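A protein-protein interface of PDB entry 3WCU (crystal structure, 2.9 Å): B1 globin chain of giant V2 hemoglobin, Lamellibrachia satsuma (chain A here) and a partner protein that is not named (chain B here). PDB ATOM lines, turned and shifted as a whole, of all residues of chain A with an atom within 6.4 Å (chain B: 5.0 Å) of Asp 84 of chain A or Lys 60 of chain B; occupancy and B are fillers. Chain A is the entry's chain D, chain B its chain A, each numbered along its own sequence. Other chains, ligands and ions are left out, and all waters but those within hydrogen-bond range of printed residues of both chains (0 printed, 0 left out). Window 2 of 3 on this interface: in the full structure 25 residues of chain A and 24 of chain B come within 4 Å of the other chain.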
ATOM      1  N   PHE A   3      14.388  -6.966   4.684  1.00  0.00           N
ATOM      2  CA  PHE A   3      15.536  -7.220   3.796  1.00  0.00           C
ATOM      3  C   PHE A   3      16.785  -6.338   3.822  1.00  0.00           C
ATOM      4  O   PHE A   3      17.874  -6.816   4.154  1.00  0.00           O
ATOM      5  CB  PHE A   3      15.049  -7.292   2.358  1.00  0.00           C
ATOM      6  CG  PHE A   3      13.966  -8.291   2.166  1.00  0.00           C
ATOM      7  CD1 PHE A   3      12.673  -8.007   2.594  1.00  0.00           C
ATOM      8  CD2 PHE A   3      14.254  -9.552   1.650  1.00  0.00           C
ATOM      9  CE1 PHE A   3      11.681  -8.962   2.528  1.00  0.00           C
ATOM     10  CE2 PHE A   3      13.270 -10.521   1.578  1.00  0.00           C
ATOM     11  CZ  PHE A   3      11.974 -10.232   2.023  1.00  0.00           C
ATOM     12  N   TYR A  81      11.883  -5.436  -6.371  1.00  0.00           N
ATOM     13  CA  TYR A  81      10.808  -5.354  -5.393  1.00  0.00           C
ATOM     14  C   TYR A  81      11.378  -5.260  -3.990  1.00  0.00           C
ATOM     15  O   TYR A  81      10.674  -5.480  -3.011  1.00  0.00           O
ATOM     16  CB  TYR A  81       9.918  -6.572  -5.498  1.00  0.00           C
ATOM     17  CG  TYR A  81       8.748  -6.369  -6.409  1.00  0.00           C
ATOM     18  CD1 TYR A  81       7.473  -6.136  -5.886  1.00  0.00           C
ATOM     19  CD2 TYR A  81       8.898  -6.426  -7.792  1.00  0.00           C
ATOM     20  CE1 TYR A  81       6.376  -5.974  -6.711  1.00  0.00           C
ATOM     21  CE2 TYR A  81       7.791  -6.262  -8.639  1.00  0.00           C
ATOM     22  CZ  TYR A  81       6.534  -6.040  -8.085  1.00  0.00           C
ATOM     23  OH  TYR A  81       5.425  -5.904  -8.896  1.00  0.00           O
ATOM     24  N   LEU A  82      12.664  -4.932  -3.909  1.00  0.00           N
ATOM     25  CA  LEU A  82      13.356  -4.797  -2.643  1.00  0.00           C
ATOM     26  C   LEU A  82      12.738  -3.737  -1.751  1.00  0.00           C
ATOM     27  O   LEU A  82      12.811  -3.838  -0.534  1.00  0.00           O
ATOM     28  CB  LEU A  82      14.827  -4.471  -2.893  1.00  0.00           C
ATOM     29  CG  LEU A  82      15.713  -5.710  -3.003  1.00  0.00           C
ATOM     30  CD1 LEU A  82      17.105  -5.364  -3.534  1.00  0.00           C
ATOM     31  CD2 LEU A  82      15.798  -6.345  -1.628  1.00  0.00           C
ATOM     32  N   ASN A  83      12.114  -2.728  -2.353  1.00  0.00           N
ATOM     33  CA  ASN A  83      11.501  -1.641  -1.586  1.00  0.00           C
ATOM     34  C   ASN A  83      10.092  -1.933  -1.118  1.00  0.00           C
ATOM     35  O   ASN A  83       9.408  -1.045  -0.634  1.00  0.00           O
ATOM     36  CB  ASN A  83      11.464  -0.357  -2.408  1.00  0.00           C
ATOM     37  CG  ASN A  83      12.832   0.091  -2.842  1.00  0.00           C
ATOM     38  OD1 ASN A  83      13.730   0.237  -2.014  1.00  0.00           O
ATOM     39  ND2 ASN A  83      13.005   0.317  -4.145  1.00  0.00           N
ATOM     40  N   ASP A  84       9.653  -3.170  -1.285  1.00  0.00           N
ATOM     41  CA  ASP A  84       8.315  -3.562  -0.881  1.00  0.00           C
ATOM     42  C   ASP A  84       8.387  -4.902  -0.179  1.00  0.00           C
ATOM     43  O   ASP A  84       8.069  -5.937  -0.770  1.00  0.00           O
ATOM     44  CB  ASP A  84       7.398  -3.676  -2.094  1.00  0.00           C
ATOM     45  CG  ASP A  84       5.984  -4.076  -1.716  1.00  0.00           C
ATOM     46  OD1 ASP A  84       5.740  -4.391  -0.533  1.00  0.00           O
ATOM     47  OD2 ASP A  84       5.106  -4.079  -2.605  1.00  0.00           O
ATOM     48  N   ALA A  85       8.813  -4.866   1.080  1.00  0.00           N
ATOM     49  CA  ALA A  85       8.940  -6.060   1.907  1.00  0.00           C
ATOM     50  C   ALA A  85       7.684  -6.919   1.828  1.00  0.00           C
ATOM     51  O   ALA A  85       7.755  -8.143   1.673  1.00  0.00           O
ATOM     52  CB  ALA A  85       9.204  -5.657   3.346  1.00  0.00           C
ATOM     53  N   GLY A  86       6.532  -6.268   1.935  1.00  0.00           N
ATOM     54  CA  GLY A  86       5.280  -6.993   1.877  1.00  0.00           C
ATOM     55  C   GLY A  86       5.258  -8.011   0.757  1.00  0.00           C
ATOM     56  O   GLY A  86       5.309  -9.219   0.992  1.00  0.00           O
ATOM     57  N   THR A  87       5.195  -7.519  -0.472  1.00  0.00           N
ATOM     58  CA  THR A  87       5.154  -8.398  -1.626  1.00  0.00           C
ATOM     59  C   THR A  87       6.405  -9.252  -1.757  1.00  0.00           C
ATOM     60  O   THR A  87       6.319 -10.421  -2.115  1.00  0.00           O
ATOM     61  CB  THR A  87       4.972  -7.605  -2.937  1.00  0.00           C
ATOM     62  OG1 THR A  87       3.798  -6.782  -2.847  1.00  0.00           O
ATOM     63  CG2 THR A  87       4.833  -8.570  -4.119  1.00  0.00           C
ATOM     64  N   LEU A  88       7.565  -8.679  -1.472  1.00  0.00           N
ATOM     65  CA  LEU A  88       8.791  -9.447  -1.601  1.00  0.00           C
ATOM     66  C   LEU A  88       8.807 -10.654  -0.684  1.00  0.00           C
ATOM     67  O   LEU A  88       9.343 -11.701  -1.047  1.00  0.00           O
ATOM     68  CB  LEU A  88      10.029  -8.589  -1.314  1.00  0.00           C
ATOM     69  CG  LEU A  88      11.343  -9.388  -1.348  1.00  0.00           C
ATOM     70  CD1 LEU A  88      11.538 -10.049  -2.701  1.00  0.00           C
ATOM     71  CD2 LEU A  88      12.493  -8.461  -1.054  1.00  0.00           C
ATOM     72  N   THR A  89       8.236 -10.519   0.505  1.00  0.00           N
ATOM     73  CA  THR A  89       8.232 -11.645   1.416  1.00  0.00           C
ATOM     74  C   THR A  89       7.438 -12.776   0.794  1.00  0.00           C
ATOM     75  O   THR A  89       7.885 -13.925   0.810  1.00  0.00           O
ATOM     76  CB  THR A  89       7.630 -11.287   2.762  1.00  0.00           C
ATOM     77  OG1 THR A  89       8.402 -10.243   3.364  1.00  0.00           O
ATOM     78  CG2 THR A  89       7.665 -12.480   3.672  1.00  0.00           C
ATOM     79  N   LEU A  91       6.720 -13.210  -2.466  1.00  0.00           N
ATOM     80  CA  LEU A  91       7.417 -13.658  -3.672  1.00  0.00           C
ATOM     81  C   LEU A  91       8.533 -14.653  -3.347  1.00  0.00           C
ATOM     82  O   LEU A  91       8.759 -15.595  -4.093  1.00  0.00           O
ATOM     83  CB  LEU A  91       8.000 -12.458  -4.441  1.00  0.00           C
ATOM     84  CG  LEU A  91       7.022 -11.560  -5.221  1.00  0.00           C
ATOM     85  CD1 LEU A  91       7.750 -10.333  -5.747  1.00  0.00           C
ATOM     86  CD2 LEU A  91       6.387 -12.343  -6.370  1.00  0.00           C
ATOM     87  N   MET B  54      -6.682  -6.195  -4.535  1.00  0.00           N
ATOM     88  CA  MET B  54      -5.516  -6.012  -5.375  1.00  0.00           C
ATOM     89  C   MET B  54      -4.281  -5.478  -4.661  1.00  0.00           C
ATOM     90  O   MET B  54      -3.167  -5.600  -5.179  1.00  0.00           O
ATOM     91  CB  MET B  54      -5.886  -5.103  -6.542  1.00  0.00           C
ATOM     92  CG  MET B  54      -6.962  -5.692  -7.419  1.00  0.00           C
ATOM     93  SD  MET B  54      -7.388  -4.680  -8.837  1.00  0.00           S
ATOM     94  CE  MET B  54      -5.885  -4.910  -9.840  1.00  0.00           C
ATOM     95  N   ARG B  55      -4.473  -4.904  -3.476  1.00  0.00           N
ATOM     96  CA  ARG B  55      -3.358  -4.347  -2.713  1.00  0.00           C
ATOM     97  C   ARG B  55      -2.724  -5.375  -1.773  1.00  0.00           C
ATOM     98  O   ARG B  55      -1.638  -5.142  -1.240  1.00  0.00           O
ATOM     99  CB  ARG B  55      -3.823  -3.132  -1.912  1.00  0.00           C
ATOM    100  CG  ARG B  55      -4.682  -2.163  -2.707  1.00  0.00           C
ATOM    101  CD  ARG B  55      -5.981  -1.865  -1.965  1.00  0.00           C
ATOM    102  NE  ARG B  55      -5.763  -0.992  -0.817  1.00  0.00           N
ATOM    103  CZ  ARG B  55      -6.547  -0.954   0.254  1.00  0.00           C
ATOM    104  NH1 ARG B  55      -6.272  -0.119   1.246  1.00  0.00           N
ATOM    105  NH2 ARG B  55      -7.591  -1.766   0.346  1.00  0.00           N
ATOM    106  N   SER B  56      -3.388  -6.510  -1.573  1.00  0.00           N
ATOM    107  CA  SER B  56      -2.855  -7.552  -0.697  1.00  0.00           C
ATOM    108  C   SER B  56      -1.551  -8.095  -1.275  1.00  0.00           C
ATOM    109  O   SER B  56      -1.484  -8.402  -2.457  1.00  0.00           O
ATOM    110  CB  SER B  56      -3.845  -8.693  -0.587  1.00  0.00           C
ATOM    111  OG  SER B  56      -3.969  -9.317  -1.846  1.00  0.00           O
ATOM    112  N   PRO B  57      -0.508  -8.254  -0.442  1.00  0.00           N
ATOM    113  CA  PRO B  57       0.773  -8.763  -0.924  1.00  0.00           C
ATOM    114  C   PRO B  57       0.649 -10.055  -1.709  1.00  0.00           C
ATOM    115  O   PRO B  57       1.514 -10.370  -2.525  1.00  0.00           O
ATOM    116  CB  PRO B  57       1.575  -8.937   0.360  1.00  0.00           C
ATOM    117  CG  PRO B  57       0.548  -9.307   1.328  1.00  0.00           C
ATOM    118  CD  PRO B  57      -0.543  -8.307   1.027  1.00  0.00           C
ATOM    119  N   GLN B  58      -0.418 -10.809  -1.460  1.00  0.00           N
ATOM    120  CA  GLN B  58      -0.624 -12.064  -2.182  1.00  0.00           C
ATOM    121  C   GLN B  58      -0.773 -11.780  -3.672  1.00  0.00           C
ATOM    122  O   GLN B  58      -0.112 -12.400  -4.509  1.00  0.00           O
ATOM    123  CB  GLN B  58      -1.886 -12.777  -1.688  1.00  0.00           C
ATOM    124  CG  GLN B  58      -1.701 -13.622  -0.445  1.00  0.00           C
ATOM    125  CD  GLN B  58      -1.219 -12.817   0.739  1.00  0.00           C
ATOM    126  OE1 GLN B  58      -1.868 -11.857   1.161  1.00  0.00           O
ATOM    127  NE2 GLN B  58      -0.070 -13.206   1.287  1.00  0.00           N
ATOM    128  N   PHE B  59      -1.644 -10.823  -3.981  1.00  0.00           N
ATOM    129  CA  PHE B  59      -1.932 -10.434  -5.354  1.00  0.00           C
ATOM    130  C   PHE B  59      -0.869  -9.543  -5.976  1.00  0.00           C
ATOM    131  O   PHE B  59      -0.654  -9.589  -7.184  1.00  0.00           O
ATOM    132  CB  PHE B  59      -3.286  -9.728  -5.426  1.00  0.00           C
ATOM    133  CG  PHE B  59      -3.785  -9.532  -6.820  1.00  0.00           C
ATOM    134  CD1 PHE B  59      -4.023  -8.256  -7.316  1.00  0.00           C
ATOM    135  CD2 PHE B  59      -4.018 -10.623  -7.643  1.00  0.00           C
ATOM    136  CE1 PHE B  59      -4.487  -8.068  -8.618  1.00  0.00           C
ATOM    137  CE2 PHE B  59      -4.481 -10.446  -8.943  1.00  0.00           C
ATOM    138  CZ  PHE B  59      -4.715  -9.164  -9.430  1.00  0.00           C
ATOM    139  N   LYS B  60      -0.220  -8.715  -5.169  1.00  0.00           N
ATOM    140  CA  LYS B  60       0.816  -7.861  -5.711  1.00  0.00           C
ATOM    141  C   LYS B  60       1.936  -8.784  -6.179  1.00  0.00           C
ATOM    142  O   LYS B  60       2.599  -8.511  -7.178  1.00  0.00           O
ATOM    143  CB  LYS B  60       1.348  -6.883  -4.654  1.00  0.00           C
ATOM    144  CG  LYS B  60       0.418  -5.716  -4.321  1.00  0.00           C
ATOM    145  CD  LYS B  60       1.114  -4.651  -3.445  1.00  0.00           C
ATOM    146  CE  LYS B  60       1.530  -5.194  -2.059  1.00  0.00           C
ATOM    147  NZ  LYS B  60       2.300  -4.233  -1.204  1.00  0.00           N
ATOM    148  N   ALA B  61       2.128  -9.886  -5.460  1.00  0.00           N
ATOM    149  CA  ALA B  61       3.164 -10.851  -5.798  1.00  0.00           C
ATOM    150  C   ALA B  61       2.807 -11.573  -7.080  1.00  0.00           C
ATOM    151  O   ALA B  61       3.691 -11.938  -7.859  1.00  0.00           O
ATOM    152  CB  ALA B  61       3.331 -11.848  -4.673  1.00  0.00           C
ATOM    153  N   HIS B  62       1.512 -11.795  -7.294  1.00  0.00           N
ATOM    154  CA  HIS B  62       1.055 -12.460  -8.510  1.00  0.00           C
ATOM    155  C   HIS B  62       1.365 -11.536  -9.678  1.00  0.00           C
ATOM    156  O   HIS B  62       1.925 -11.958 -10.686  1.00  0.00           O
ATOM    157  CB  HIS B  62      -0.452 -12.739  -8.454  1.00  0.00           C
ATOM    158  CG  HIS B  62      -1.027 -13.226  -9.750  1.00  0.00           C
ATOM    159  ND1 HIS B  62      -0.641 -14.409 -10.339  1.00  0.00           N
ATOM    160  CD2 HIS B  62      -1.947 -12.677 -10.580  1.00  0.00           C
ATOM    161  CE1 HIS B  62      -1.295 -14.566 -11.476  1.00  0.00           C
ATOM    162  NE2 HIS B  62      -2.094 -13.529 -11.646  1.00  0.00           N
ATOM    163  N   ILE B  63       0.995 -10.268  -9.533  1.00  0.00           N
ATOM    164  CA  ILE B  63       1.259  -9.295 -10.576  1.00  0.00           C
ATOM    165  C   ILE B  63       2.750  -9.322 -10.865  1.00  0.00           C
ATOM    166  O   ILE B  63       3.166  -9.326 -12.018  1.00  0.00           O
ATOM    167  CB  ILE B  63       0.884  -7.865 -10.141  1.00  0.00           C
ATOM    168  CG1 ILE B  63      -0.596  -7.799  -9.761  1.00  0.00           C
ATOM    169  CG2 ILE B  63       1.185  -6.892 -11.272  1.00  0.00           C
ATOM    170  CD1 ILE B  63      -1.102  -6.397  -9.489  1.00  0.00           C
ATOM    171  N   ALA B  64       3.550  -9.350  -9.805  1.00  0.00           N
ATOM    172  CA  ALA B  64       4.996  -9.366  -9.940  1.00  0.00           C
ATOM    173  C   ALA B  64       5.455 -10.579 -10.722  1.00  0.00           C
ATOM    174  O   ALA B  64       6.399 -10.491 -11.508  1.00  0.00           O
ATOM    175  CB  ALA B  64       5.654  -9.357  -8.572  1.00  0.00           C
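The side-chain carboxylate of Asp 84 of chain A is in salt-bridge range of the side-chain amino group of Lys 60 of chain B. The side-chain hydroxyl (OG1) of Thr 87 of chain A sits close to the side-chain amino group (NZ) of Lys 60 of chain B.
The side-chain carboxylate of Asp 84 of chain A lies close to the backbone NH of Gly 86 of chain A, at 3.2 Å. OD2 of Asp 84 of chain A is in hydrogen-bond range of OG1 of Thr 87 of chain A (3.0 Å).
Ala 64 of chain B touches Tyr 81 of chain A. O of Gly 86 of chain A touches CB of Pro 57 of chain B (3.8 Å). Pro 57 of chain B touches Thr 87 of chain A. Thr 87 of chain A touches Ala 61 of chain B (CG2 to CA, 3.3 Å). CD2 of Leu 91 of chain A touches O of Ala 61 of chain B, at 3.1 Å. Ala 64 of chain B touches Leu 91 of chain A (CB to CD1, 3.7 Å).
Asp 84 of chain A touches just one residue of chain B: Lys 60. Of the printed residues of chain B, Gly 86 of chain A touches Pro 57. Of the printed residues of chain B, Thr 87 of chain A touches Pro 57, Lys 60 and Ala 61. Printed residues of chain A within 4 Å of Pro 57 of chain B: Gly 86 and Thr 87. Lys 60 of chain B touches two residues of chain A. Printed residues of chain A within 4 Å of Ala 61 of chain B: Thr 87 and Leu 91. Printed residues of chain A within 4 Å of Ala 64 of chain B: Tyr 81 and Leu 91. The nearest residue of chain A that does not touch Lys 60 of chain B is Tyr 81 of chain A (4.2 Å). The nearest printed residue of chain B that does not touch Gly 86 of chain A is Lys 60 of chain B (5.1 Å).
Of the 11 printed residues of chain B, 4 touch a printed residue of chain A. Of the 11 printed residues of chain A, 5 touch a printed residue of chain B. Printed residues of chain A that touch a printed residue of chain B: Tyr 81, Asp 84, Gly 86, Thr 87 and Leu 91. Among the printed residues, 8 pairs touch across the chains. Among the printed residues, Asp or Glu carboxylates within 4 Å of a Lys or Arg side-chain nitrogen of the other chain: Asp 84 of chain A with Lys 60 of chain B.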
